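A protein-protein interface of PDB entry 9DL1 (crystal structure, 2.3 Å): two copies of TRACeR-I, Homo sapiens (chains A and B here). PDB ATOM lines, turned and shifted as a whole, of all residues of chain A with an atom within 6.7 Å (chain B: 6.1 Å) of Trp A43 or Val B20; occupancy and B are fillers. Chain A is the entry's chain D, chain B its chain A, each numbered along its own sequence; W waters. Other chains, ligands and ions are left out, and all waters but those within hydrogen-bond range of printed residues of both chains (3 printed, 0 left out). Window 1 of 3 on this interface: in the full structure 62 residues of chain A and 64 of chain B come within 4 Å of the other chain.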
ATOM      1  N   MET A  12      -2.937 -36.465  15.823  1.00  0.00           N
ATOM      2  CA  MET A  12      -4.044 -36.252  16.788  1.00  0.00           C
ATOM      3  C   MET A  12      -4.843 -35.006  16.396  1.00  0.00           C
ATOM      4  O   MET A  12      -6.068 -35.030  16.515  1.00  0.00           O
ATOM      5  CB  MET A  12      -3.489 -36.093  18.204  1.00  0.00           C
ATOM      6  CG  MET A  12      -4.449 -35.475  19.177  1.00  0.00           C
ATOM      7  SD  MET A  12      -4.300 -36.160  20.836  1.00  0.00           S
ATOM      8  CE  MET A  12      -6.004 -35.993  21.356  1.00  0.00           C
ATOM      9  N   LEU A  16      -8.942 -35.206  15.617  1.00  0.00           N
ATOM     10  CA  LEU A  16     -10.008 -34.434  16.248  1.00  0.00           C
ATOM     11  C   LEU A  16     -10.735 -33.551  15.248  1.00  0.00           C
ATOM     12  O   LEU A  16     -11.935 -33.302  15.410  1.00  0.00           O
ATOM     13  CB  LEU A  16      -9.452 -33.578  17.386  1.00  0.00           C
ATOM     14  CG  LEU A  16      -8.892 -34.427  18.519  1.00  0.00           C
ATOM     15  CD1 LEU A  16      -8.180 -33.567  19.549  1.00  0.00           C
ATOM     16  CD2 LEU A  16     -10.004 -35.253  19.143  1.00  0.00           C
ATOM     17  N   VAL A  20     -14.759 -33.112  14.911  1.00  0.00           N
ATOM     18  CA  VAL A  20     -15.507 -31.860  14.824  1.00  0.00           C
ATOM     19  C   VAL A  20     -16.300 -31.797  13.521  1.00  0.00           C
ATOM     20  O   VAL A  20     -17.513 -31.556  13.523  1.00  0.00           O
ATOM     21  CB  VAL A  20     -14.558 -30.649  14.955  1.00  0.00           C
ATOM     22  CG1 VAL A  20     -15.343 -29.348  14.840  1.00  0.00           C
ATOM     23  CG2 VAL A  20     -13.748 -30.705  16.280  1.00  0.00           C
ATOM     24  N   ILE A  38     -15.401 -23.244  15.964  1.00  0.00           N
ATOM     25  CA  ILE A  38     -14.226 -22.383  15.859  1.00  0.00           C
ATOM     26  C   ILE A  38     -13.447 -22.391  17.176  1.00  0.00           C
ATOM     27  O   ILE A  38     -12.219 -22.534  17.193  1.00  0.00           O
ATOM     28  CB  ILE A  38     -14.641 -20.956  15.438  1.00  0.00           C
ATOM     29  CG1 ILE A  38     -14.802 -20.857  13.922  1.00  0.00           C
ATOM     30  CG2 ILE A  38     -13.620 -19.940  15.845  1.00  0.00           C
ATOM     31  CD1 ILE A  38     -15.683 -19.675  13.475  1.00  0.00           C
ATOM     32  N   ARG A  39     -14.152 -22.258  18.306  1.00  0.00           N
ATOM     33  CA  ARG A  39     -13.474 -22.327  19.599  1.00  0.00           C
ATOM     34  C   ARG A  39     -12.884 -23.711  19.867  1.00  0.00           C
ATOM     35  O   ARG A  39     -11.814 -23.819  20.481  1.00  0.00           O
ATOM     36  CB  ARG A  39     -14.427 -21.949  20.729  1.00  0.00           C
ATOM     37  CG  ARG A  39     -14.650 -20.455  20.854  1.00  0.00           C
ATOM     38  CD  ARG A  39     -15.834 -20.160  21.735  1.00  0.00           C
ATOM     39  NE  ARG A  39     -15.399 -19.939  23.109  1.00  0.00           N
ATOM     40  CZ  ARG A  39     -16.220 -19.843  24.150  1.00  0.00           C
ATOM     41  NH1 ARG A  39     -17.536 -19.935  24.001  1.00  0.00           N
ATOM     42  NH2 ARG A  39     -15.709 -19.660  25.369  1.00  0.00           N
ATOM     43  N   VAL A  40     -13.547 -24.774  19.410  1.00  0.00           N
ATOM     44  CA  VAL A  40     -12.974 -26.104  19.587  1.00  0.00           C
ATOM     45  C   VAL A  40     -11.683 -26.244  18.785  1.00  0.00           C
ATOM     46  O   VAL A  40     -10.710 -26.845  19.255  1.00  0.00           O
ATOM     47  CB  VAL A  40     -14.001 -27.191  19.216  1.00  0.00           C
ATOM     48  CG1 VAL A  40     -13.369 -28.565  19.319  1.00  0.00           C
ATOM     49  CG2 VAL A  40     -15.212 -27.101  20.122  1.00  0.00           C
ATOM     50  N   LEU A  41     -11.634 -25.702  17.578  1.00  0.00           N
ATOM     51  CA  LEU A  41     -10.402 -25.788  16.763  1.00  0.00           C
ATOM     52  C   LEU A  41      -9.292 -24.999  17.472  1.00  0.00           C
ATOM     53  O   LEU A  41      -8.152 -25.446  17.420  1.00  0.00           O
ATOM     54  CB  LEU A  41     -10.645 -25.259  15.342  1.00  0.00           C
ATOM     55  CG  LEU A  41     -11.670 -25.979  14.468  1.00  0.00           C
ATOM     56  CD1 LEU A  41     -11.338 -25.787  13.000  1.00  0.00           C
ATOM     57  CD2 LEU A  41     -11.771 -27.454  14.804  1.00  0.00           C
ATOM     58  N   ASP A  42      -9.634 -23.861  18.082  1.00  0.00           N
ATOM     59  CA  ASP A  42      -8.647 -23.095  18.845  1.00  0.00           C
ATOM     60  C   ASP A  42      -8.076 -23.921  19.996  1.00  0.00           C
ATOM     61  O   ASP A  42      -6.867 -23.883  20.265  1.00  0.00           O
ATOM     62  CB  ASP A  42      -9.283 -21.820  19.397  1.00  0.00           C
ATOM     63  CG  ASP A  42      -9.271 -20.686  18.411  1.00  0.00           C
ATOM     64  OD1 ASP A  42      -8.288 -20.571  17.656  1.00  0.00           O
ATOM     65  OD2 ASP A  42     -10.247 -19.905  18.392  1.00  0.00           O
ATOM     66  N   TRP A  43      -8.943 -24.663  20.689  1.00  0.00           N
ATOM     67  CA  TRP A  43      -8.511 -25.503  21.795  1.00  0.00           C
ATOM     68  C   TRP A  43      -7.620 -26.638  21.306  1.00  0.00           C
ATOM     69  O   TRP A  43      -6.589 -26.935  21.922  1.00  0.00           O
ATOM     70  CB  TRP A  43      -9.751 -26.030  22.545  1.00  0.00           C
ATOM     71  CG  TRP A  43      -9.512 -27.212  23.453  1.00  0.00           C
ATOM     72  CD1 TRP A  43      -8.946 -27.200  24.705  1.00  0.00           C
ATOM     73  CD2 TRP A  43      -9.861 -28.579  23.187  1.00  0.00           C
ATOM     74  NE1 TRP A  43      -8.911 -28.478  25.225  1.00  0.00           N
ATOM     75  CE2 TRP A  43      -9.459 -29.343  24.311  1.00  0.00           C
ATOM     76  CE3 TRP A  43     -10.465 -29.234  22.106  1.00  0.00           C
ATOM     77  CZ2 TRP A  43      -9.645 -30.735  24.378  1.00  0.00           C
ATOM     78  CZ3 TRP A  43     -10.654 -30.613  22.179  1.00  0.00           C
ATOM     79  CH2 TRP A  43     -10.248 -31.346  23.310  1.00  0.00           C
ATOM     80  N   ILE A  44      -8.004 -27.277  20.196  1.00  0.00           N
ATOM     81  CA  ILE A  44      -7.160 -28.304  19.591  1.00  0.00           C
ATOM     82  C   ILE A  44      -5.765 -27.752  19.322  1.00  0.00           C
ATOM     83  O   ILE A  44      -4.754 -28.363  19.691  1.00  0.00           O
ATOM     84  CB  ILE A  44      -7.808 -28.846  18.302  1.00  0.00           C
ATOM     85  CG1 ILE A  44      -9.131 -29.555  18.604  1.00  0.00           C
ATOM     86  CG2 ILE A  44      -6.882 -29.825  17.627  1.00  0.00           C
ATOM     87  CD1 ILE A  44      -9.913 -29.938  17.338  1.00  0.00           C
ATOM     88  N   MET A  45      -5.690 -26.579  18.683  1.00  0.00           N
ATOM     89  CA  MET A  45      -4.395 -25.965  18.398  1.00  0.00           C
ATOM     90  C   MET A  45      -3.655 -25.606  19.685  1.00  0.00           C
ATOM     91  O   MET A  45      -2.448 -25.853  19.810  1.00  0.00           O
ATOM     92  CB  MET A  45      -4.578 -24.719  17.520  1.00  0.00           C
ATOM     93  CG  MET A  45      -4.934 -25.004  16.064  1.00  0.00           C
ATOM     94  SD  MET A  45      -4.803 -23.545  14.996  1.00  0.00           S
ATOM     95  CE  MET A  45      -6.455 -22.862  15.202  1.00  0.00           C
ATOM     96  N   ALA A  46      -4.352 -25.018  20.654  1.00  0.00           N
ATOM     97  CA  ALA A  46      -3.689 -24.663  21.904  1.00  0.00           C
ATOM     98  C   ALA A  46      -3.145 -25.896  22.616  1.00  0.00           C
ATOM     99  O   ALA A  46      -2.039 -25.865  23.165  1.00  0.00           O
ATOM    100  CB  ALA A  46      -4.651 -23.893  22.816  1.00  0.00           C
ATOM    101  N   GLU A  47      -3.910 -26.987  22.634  1.00  0.00           N
ATOM    102  CA  GLU A  47      -3.461 -28.159  23.377  1.00  0.00           C
ATOM    103  C   GLU A  47      -2.298 -28.838  22.678  1.00  0.00           C
ATOM    104  O   GLU A  47      -1.389 -29.353  23.338  1.00  0.00           O
ATOM    105  CB  GLU A  47      -4.609 -29.136  23.574  1.00  0.00           C
ATOM    106  CG  GLU A  47      -5.636 -28.677  24.580  1.00  0.00           C
ATOM    107  CD  GLU A  47      -5.016 -28.172  25.891  1.00  0.00           C
ATOM    108  OE1 GLU A  47      -3.954 -28.685  26.337  1.00  0.00           O
ATOM    109  OE2 GLU A  47      -5.614 -27.267  26.493  1.00  0.00           O
ATOM    110  N   ALA A  48      -2.306 -28.844  21.342  1.00  0.00           N
ATOM    111  CA  ALA A  48      -1.133 -29.288  20.599  1.00  0.00           C
ATOM    112  C   ALA A  48       0.102 -28.489  20.996  1.00  0.00           C
ATOM    113  O   ALA A  48       1.176 -29.060  21.225  1.00  0.00           O
ATOM    114  CB  ALA A  48      -1.393 -29.164  19.098  1.00  0.00           C
ATOM    115  N   ASP A  49      -0.036 -27.165  21.090  1.00  0.00           N
ATOM    116  CA  ASP A  49       1.089 -26.334  21.505  1.00  0.00           C
ATOM    117  C   ASP A  49       1.572 -26.708  22.899  1.00  0.00           C
ATOM    118  O   ASP A  49       2.780 -26.731  23.157  1.00  0.00           O
ATOM    119  CB  ASP A  49       0.697 -24.861  21.465  1.00  0.00           C
ATOM    120  CG  ASP A  49       0.764 -24.286  20.071  1.00  0.00           C
ATOM    121  OD1 ASP A  49       1.552 -24.820  19.261  1.00  0.00           O
ATOM    122  OD2 ASP A  49       0.026 -23.313  19.788  1.00  0.00           O
ATOM    123  N   ASN A  50       0.640 -26.996  23.812  1.00  0.00           N
ATOM    124  CA  ASN A  50       1.031 -27.392  25.157  1.00  0.00           C
ATOM    125  C   ASN A  50       1.823 -28.694  25.122  1.00  0.00           C
ATOM    126  O   ASN A  50       2.840 -28.836  25.817  1.00  0.00           O
ATOM    127  CB  ASN A  50      -0.214 -27.526  26.044  1.00  0.00           C
ATOM    128  CG  ASN A  50      -0.802 -26.170  26.436  1.00  0.00           C
ATOM    129  OD1 ASN A  50      -0.071 -25.222  26.715  1.00  0.00           O
ATOM    130  ND2 ASN A  50      -2.127 -26.077  26.447  1.00  0.00           N
ATOM    131  N   LEU A  76      -9.534 -29.703  40.535  1.00  0.00           N
ATOM    132  CA  LEU A  76     -10.626 -30.489  39.983  1.00  0.00           C
ATOM    133  C   LEU A  76     -10.969 -31.663  40.887  1.00  0.00           C
ATOM    134  O   LEU A  76     -12.148 -31.971  41.093  1.00  0.00           O
ATOM    135  CB  LEU A  76     -10.254 -30.970  38.583  1.00  0.00           C
ATOM    136  CG  LEU A  76     -10.963 -30.182  37.490  1.00  0.00           C
ATOM    137  CD1 LEU A  76      -9.969 -29.664  36.437  1.00  0.00           C
ATOM    138  CD2 LEU A  76     -12.038 -31.047  36.866  1.00  0.00           C
ATOM    139  N   PHE A 105     -20.815 -27.945  36.689  1.00  0.00           N
ATOM    140  CA  PHE A 105     -19.640 -28.652  36.202  1.00  0.00           C
ATOM    141  C   PHE A 105     -19.500 -30.009  36.886  1.00  0.00           C
ATOM    142  O   PHE A 105     -19.311 -31.033  36.219  1.00  0.00           O
ATOM    143  CB  PHE A 105     -18.386 -27.801  36.402  1.00  0.00           C
ATOM    144  CG  PHE A 105     -17.147 -28.448  35.871  1.00  0.00           C
ATOM    145  CD1 PHE A 105     -16.860 -28.416  34.515  1.00  0.00           C
ATOM    146  CD2 PHE A 105     -16.297 -29.144  36.714  1.00  0.00           C
ATOM    147  CE1 PHE A 105     -15.735 -29.036  34.019  1.00  0.00           C
ATOM    148  CE2 PHE A 105     -15.167 -29.763  36.220  1.00  0.00           C
ATOM    149  CZ  PHE A 105     -14.887 -29.708  34.876  1.00  0.00           C
ATOM    150  N   MET B  15      -9.247 -40.027  27.683  1.00  0.00           N
ATOM    151  CA  MET B  15      -8.106 -39.345  27.081  1.00  0.00           C
ATOM    152  C   MET B  15      -8.440 -37.882  26.778  1.00  0.00           C
ATOM    153  O   MET B  15      -7.658 -36.971  27.093  1.00  0.00           O
ATOM    154  CB  MET B  15      -7.658 -40.115  25.828  1.00  0.00           C
ATOM    155  CG  MET B  15      -6.434 -39.565  25.129  1.00  0.00           C
ATOM    156  SD  MET B  15      -6.745 -38.119  24.070  1.00  0.00           S
ATOM    157  CE  MET B  15      -7.601 -38.860  22.667  1.00  0.00           C
ATOM    158  N   LEU B  16      -9.612 -37.634  26.190  1.00  0.00           N
ATOM    159  CA  LEU B  16     -10.027 -36.256  25.929  1.00  0.00           C
ATOM    160  C   LEU B  16     -10.407 -35.511  27.210  1.00  0.00           C
ATOM    161  O   LEU B  16     -10.240 -34.286  27.282  1.00  0.00           O
ATOM    162  CB  LEU B  16     -11.189 -36.239  24.938  1.00  0.00           C
ATOM    163  CG  LEU B  16     -10.810 -36.694  23.522  1.00  0.00           C
ATOM    164  CD1 LEU B  16     -11.987 -36.614  22.571  1.00  0.00           C
ATOM    165  CD2 LEU B  16      -9.670 -35.845  23.035  1.00  0.00           C
ATOM    166  N   LEU B  17     -10.915 -36.214  28.227  1.00  0.00           N
ATOM    167  CA  LEU B  17     -11.266 -35.528  29.463  1.00  0.00           C
ATOM    168  C   LEU B  17     -10.035 -34.890  30.097  1.00  0.00           C
ATOM    169  O   LEU B  17     -10.088 -33.745  30.555  1.00  0.00           O
ATOM    170  CB  LEU B  17     -11.945 -36.496  30.430  1.00  0.00           C
ATOM    171  CG  LEU B  17     -12.745 -35.911  31.597  1.00  0.00           C
ATOM    172  CD1 LEU B  17     -13.983 -35.163  31.101  1.00  0.00           C
ATOM    173  CD2 LEU B  17     -13.127 -37.016  32.603  1.00  0.00           C
ATOM    174  N   TRP B  18      -8.910 -35.607  30.105  1.00  0.00           N
ATOM    175  CA  TRP B  18      -7.663 -35.026  30.579  1.00  0.00           C
ATOM    176  C   TRP B  18      -7.329 -33.756  29.818  1.00  0.00           C
ATOM    177  O   TRP B  18      -6.964 -32.734  30.418  1.00  0.00           O
ATOM    178  CB  TRP B  18      -6.515 -36.019  30.428  1.00  0.00           C
ATOM    179  CG  TRP B  18      -5.185 -35.435  30.858  1.00  0.00           C
ATOM    180  CD1 TRP B  18      -4.001 -35.510  30.183  1.00  0.00           C
ATOM    181  CD2 TRP B  18      -4.909 -34.722  32.068  1.00  0.00           C
ATOM    182  NE1 TRP B  18      -3.002 -34.895  30.903  1.00  0.00           N
ATOM    183  CE2 TRP B  18      -3.538 -34.400  32.062  1.00  0.00           C
ATOM    184  CE3 TRP B  18      -5.691 -34.333  33.169  1.00  0.00           C
ATOM    185  CZ2 TRP B  18      -2.929 -33.690  33.105  1.00  0.00           C
ATOM    186  CZ3 TRP B  18      -5.086 -33.621  34.197  1.00  0.00           C
ATOM    187  CH2 TRP B  18      -3.719 -33.306  34.154  1.00  0.00           C
ATOM    188  N   ARG B  19      -7.432 -33.808  28.483  1.00  0.00           N
ATOM    189  CA  ARG B  19      -7.069 -32.654  27.678  1.00  0.00           C
ATOM    190  C   ARG B  19      -7.975 -31.471  27.967  1.00  0.00           C
ATOM    191  O   ARG B  19      -7.543 -30.324  27.851  1.00  0.00           O
ATOM    192  CB  ARG B  19      -7.105 -33.016  26.200  1.00  0.00           C
ATOM    193  CG  ARG B  19      -6.044 -34.008  25.836  1.00  0.00           C
ATOM    194  CD  ARG B  19      -6.022 -34.243  24.357  1.00  0.00           C
ATOM    195  NE  ARG B  19      -5.294 -33.217  23.620  1.00  0.00           N
ATOM    196  CZ  ARG B  19      -3.975 -33.192  23.482  1.00  0.00           C
ATOM    197  NH1 ARG B  19      -3.200 -34.085  24.081  1.00  0.00           N
ATOM    198  NH2 ARG B  19      -3.422 -32.269  22.705  1.00  0.00           N
ATOM    199  N   VAL B  20      -9.219 -31.724  28.364  1.00  0.00           N
ATOM    200  CA  VAL B  20     -10.086 -30.632  28.795  1.00  0.00           C
ATOM    201  C   VAL B  20      -9.726 -30.175  30.216  1.00  0.00           C
ATOM    202  O   VAL B  20      -9.639 -28.973  30.488  1.00  0.00           O
ATOM    203  CB  VAL B  20     -11.558 -31.073  28.689  1.00  0.00           C
ATOM    204  CG1 VAL B  20     -12.481 -29.998  29.238  1.00  0.00           C
ATOM    205  CG2 VAL B  20     -11.911 -31.435  27.256  1.00  0.00           C
ATOM    206  N   PHE B  21      -9.500 -31.126  31.137  1.00  0.00           N
ATOM    207  CA  PHE B  21      -9.223 -30.802  32.539  1.00  0.00           C
ATOM    208  C   PHE B  21      -7.942 -29.996  32.690  1.00  0.00           C
ATOM    209  O   PHE B  21      -7.888 -29.034  33.472  1.00  0.00           O
ATOM    210  CB  PHE B  21      -9.072 -32.085  33.377  1.00  0.00           C
ATOM    211  CG  PHE B  21     -10.361 -32.681  33.866  1.00  0.00           C
ATOM    212  CD1 PHE B  21     -11.577 -32.337  33.292  1.00  0.00           C
ATOM    213  CD2 PHE B  21     -10.347 -33.616  34.898  1.00  0.00           C
ATOM    214  CE1 PHE B  21     -12.765 -32.895  33.743  1.00  0.00           C
ATOM    215  CE2 PHE B  21     -11.520 -34.187  35.352  1.00  0.00           C
ATOM    216  CZ  PHE B  21     -12.739 -33.830  34.768  1.00  0.00           C
ATOM    217  N   ARG B  22      -6.886 -30.405  31.978  1.00  0.00           N
ATOM    218  CA  ARG B  22      -5.530 -30.011  32.345  1.00  0.00           C
ATOM    219  C   ARG B  22      -5.286 -28.511  32.189  1.00  0.00           C
ATOM    220  O   ARG B  22      -4.428 -27.963  32.896  1.00  0.00           O
ATOM    221  CB  ARG B  22      -4.513 -30.835  31.531  1.00  0.00           C
ATOM    222  CG  ARG B  22      -4.464 -30.514  30.036  1.00  0.00           C
ATOM    223  CD  ARG B  22      -3.555 -31.467  29.268  1.00  0.00           C
ATOM    224  NE  ARG B  22      -3.355 -30.959  27.918  1.00  0.00           N
ATOM    225  CZ  ARG B  22      -2.491 -31.437  27.031  1.00  0.00           C
ATOM    226  NH1 ARG B  22      -1.713 -32.473  27.305  1.00  0.00           N
ATOM    227  NH2 ARG B  22      -2.414 -30.865  25.836  1.00  0.00           N
ATOM    228  N   SER B  23      -6.040 -27.821  31.330  1.00  0.00           N
ATOM    229  CA  SER B  23      -5.814 -26.398  31.101  1.00  0.00           C
ATOM    230  C   SER B  23      -6.878 -25.494  31.716  1.00  0.00           C
ATOM    231  O   SER B  23      -6.758 -24.261  31.639  1.00  0.00           O
ATOM    232  CB  SER B  23      -5.700 -26.133  29.593  1.00  0.00           C
ATOM    233  OG  SER B  23      -4.499 -26.698  29.087  1.00  0.00           O
ATOM    234  N   GLN B  24      -7.893 -26.063  32.353  1.00  0.00           N
ATOM    235  CA  GLN B  24      -9.006 -25.287  32.888  1.00  0.00           C
ATOM    236  C   GLN B  24      -8.684 -24.794  34.296  1.00  0.00           C
ATOM    237  O   GLN B  24      -8.815 -25.542  35.268  1.00  0.00           O
ATOM    238  CB  GLN B  24     -10.271 -26.131  32.889  1.00  0.00           C
ATOM    239  CG  GLN B  24     -11.525 -25.373  33.265  1.00  0.00           C
ATOM    240  CD  GLN B  24     -12.689 -26.317  33.449  1.00  0.00           C
ATOM    241  OE1 GLN B  24     -13.727 -26.163  32.812  1.00  0.00           O
ATOM    242  NE2 GLN B  24     -12.513 -27.321  34.305  1.00  0.00           N
ATOM    243  N   PHE B  36     -17.996 -23.394  28.336  1.00  0.00           N
ATOM    244  CA  PHE B  36     -17.542 -23.995  27.094  1.00  0.00           C
ATOM    245  C   PHE B  36     -17.160 -25.460  27.309  1.00  0.00           C
ATOM    246  O   PHE B  36     -17.588 -26.349  26.561  1.00  0.00           O
ATOM    247  CB  PHE B  36     -16.371 -23.174  26.549  1.00  0.00           C
ATOM    248  CG  PHE B  36     -15.705 -23.777  25.346  1.00  0.00           C
ATOM    249  CD1 PHE B  36     -16.294 -23.694  24.095  1.00  0.00           C
ATOM    250  CD2 PHE B  36     -14.480 -24.418  25.466  1.00  0.00           C
ATOM    251  CE1 PHE B  36     -15.678 -24.262  22.975  1.00  0.00           C
ATOM    252  CE2 PHE B  36     -13.854 -24.970  24.366  1.00  0.00           C
ATOM    253  CZ  PHE B  36     -14.455 -24.893  23.110  1.00  0.00           C
ATOM    254  N   ASN B  37     -16.396 -25.732  28.368  1.00  0.00           N
ATOM    255  CA  ASN B  37     -15.912 -27.085  28.599  1.00  0.00           C
ATOM    256  C   ASN B  37     -17.038 -28.048  28.940  1.00  0.00           C
ATOM    257  O   ASN B  37     -16.939 -29.243  28.634  1.00  0.00           O
ATOM    258  CB  ASN B  37     -14.854 -27.079  29.699  1.00  0.00           C
ATOM    259  CG  ASN B  37     -13.499 -26.649  29.173  1.00  0.00           C
ATOM    260  OD1 ASN B  37     -13.306 -26.577  27.957  1.00  0.00           O
ATOM    261  ND2 ASN B  37     -12.563 -26.342  30.073  1.00  0.00           N
ATOM    262  N   VAL B  40     -18.188 -29.067  25.659  1.00  0.00           N
ATOM    263  CA  VAL B  40     -17.221 -29.994  25.065  1.00  0.00           C
ATOM    264  C   VAL B  40     -17.409 -31.386  25.648  1.00  0.00           C
ATOM    265  O   VAL B  40     -17.264 -32.394  24.948  1.00  0.00           O
ATOM    266  CB  VAL B  40     -15.774 -29.497  25.271  1.00  0.00           C
ATOM    267  CG1 VAL B  40     -14.779 -30.503  24.714  1.00  0.00           C
ATOM    268  CG2 VAL B  40     -15.549 -28.115  24.644  1.00  0.00           C
ATOM    269  N   LEU B  41     -17.746 -31.463  26.941  1.00  0.00           N
ATOM    270  CA  LEU B  41     -18.013 -32.751  27.565  1.00  0.00           C
ATOM    271  C   LEU B  41     -19.274 -33.388  26.990  1.00  0.00           C
ATOM    272  O   LEU B  41     -19.287 -34.589  26.702  1.00  0.00           O
ATOM    273  CB  LEU B  41     -18.099 -32.588  29.090  1.00  0.00           C
ATOM    274  CG  LEU B  41     -16.922 -33.096  29.954  1.00  0.00           C
ATOM    275  CD1 LEU B  41     -15.666 -32.270  29.782  1.00  0.00           C
ATOM    276  CD2 LEU B  41     -17.276 -33.142  31.433  1.00  0.00           C
ATOM    277  N   TRP B  43     -20.183 -32.840  23.968  1.00  0.00           N
ATOM    278  CA  TRP B  43     -19.755 -33.212  22.625  1.00  0.00           C
ATOM    279  C   TRP B  43     -19.016 -34.551  22.626  1.00  0.00           C
ATOM    280  O   TRP B  43     -19.281 -35.410  21.779  1.00  0.00           O
ATOM    281  CB  TRP B  43     -18.898 -32.088  22.025  1.00  0.00           C
ATOM    282  CG  TRP B  43     -18.231 -32.466  20.753  1.00  0.00           C
ATOM    283  CD1 TRP B  43     -18.818 -32.599  19.532  1.00  0.00           C
ATOM    284  CD2 TRP B  43     -16.842 -32.777  20.569  1.00  0.00           C
ATOM    285  NE1 TRP B  43     -17.882 -32.975  18.594  1.00  0.00           N
ATOM    286  CE2 TRP B  43     -16.662 -33.093  19.205  1.00  0.00           C
ATOM    287  CE3 TRP B  43     -15.731 -32.813  21.424  1.00  0.00           C
ATOM    288  CZ2 TRP B  43     -15.422 -33.433  18.671  1.00  0.00           C
ATOM    289  CZ3 TRP B  43     -14.487 -33.163  20.891  1.00  0.00           C
ATOM    290  CH2 TRP B  43     -14.350 -33.469  19.521  1.00  0.00           C
ATOM    291  N   ILE B  44     -18.090 -34.745  23.572  1.00  0.00           N
ATOM    292  CA  ILE B  44     -17.349 -36.003  23.656  1.00  0.00           C
ATOM    293  C   ILE B  44     -18.305 -37.173  23.846  1.00  0.00           C
ATOM    294  O   ILE B  44     -18.139 -38.235  23.230  1.00  0.00           O
ATOM    295  CB  ILE B  44     -16.317 -35.936  24.795  1.00  0.00           C
ATOM    296  CG1 ILE B  44     -15.230 -34.917  24.480  1.00  0.00           C
ATOM    297  CG2 ILE B  44     -15.712 -37.326  25.109  1.00  0.00           C
ATOM    298  CD1 ILE B  44     -14.364 -34.585  25.712  1.00  0.00           C
HETATM  299  O   HOH W   1      -4.822 -31.076  20.334  1.00  0.00           O
HETATM  300  O   HOH W   2      -2.054 -26.742  29.729  1.00  0.00           O
HETATM  301  O   HOH W   3      -1.320 -34.395  21.024  1.00  0.00           O
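Leu A16 touches its own counterpart, Leu B16.
Val A20 touches Trp B43, and with the chains exchanged Trp A43 touches Val B20.
Positions printed for both chains: 16, 20, 40, 41, 43 and 44.
Of the 16 printed residues of chain B, 10 touch a printed residue of chain A.
Among the printed residues, Asp or Glu carboxylates within 4 Å of a Lys or Arg side-chain nitrogen of the other chain: Glu A47 with Arg B22 (2.7 Å).
Water W2 bridges OG of Ser B23 (2.5 Å) and ND2 of Asn A50 (3.3 Å).
Water W1 lies within hydrogen-bond range of O of Ile A44 (2.8 Å) and NH2 of Arg B19 (3.0 Å).
Water W3 lies within hydrogen-bond range of the guanidinium group (NH2) of Arg B19 (3.4 Å) and the side-chain sulfur (SD) of Met A12 (3.5 Å).
The side-chain carboxylate (OE1) of Glu A47 is in salt-bridge range of the guanidinium group (NH2) of Arg B22 (2.7 Å).
The backbone carbonyl oxygen of Arg B19 sits at hydrogen-bond distance from the indole nitrogen of Trp A43, at 3.5 Å.
The side-chain hydroxyl (OG) of Ser B23 sits at hydrogen-bond distance from the side-chain carboxylate (OE2) of Glu A47 (2.9 Å).
The backbone carbonyl oxygen (O) of Ala A46 sits at hydrogen-bond distance from the side-chain amide nitrogen (ND2) of Asn A50 (3.3 Å).
OE1 of Glu A47 lies within hydrogen-bond range of ND2 of Asn A50.
The side-chain amide oxygen of Gln B24 is in hydrogen-bond range of the side-chain amide nitrogen of Asn B37 (3.0 Å).
Trp A43 touches just these residues of chain B: Arg B19 and Val B20.
Printed residues of chain B within 4 Å of Val A20: Trp B43 (3.8 Å).
Of the printed residues of chain B, Arg A39 touches Phe B36.
Printed residues of chain B within 4 Å of Glu A47: Arg B19, Arg B22 and Ser B23.
Printed residues of chain B within 4 Å of Phe A105: Phe B21 and Gln B24.
The nearest residue of chain B that does not touch Trp A43 is Leu B16 (4.5 Å).
Met B15 touches Met A12.
CE of Met A12 touches CD of Arg B19 (3.5 Å).
CD2 of Leu B16 touches CD2 of Leu A16, 3.95 Å away.
Val A20 touches Trp B43.
CB of Arg A39 touches CE1 of Phe B36, 3.5 Å away.
Val B20 touches Trp A43 (CG2 to CZ2, 3.7 Å).
N of Ala A48 touches NH2 of Arg B19 (3.9 Å).
Asn A50 touches Ser B23.
Leu A76 touches Phe B21.
Phe A105 touches Gln B24.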
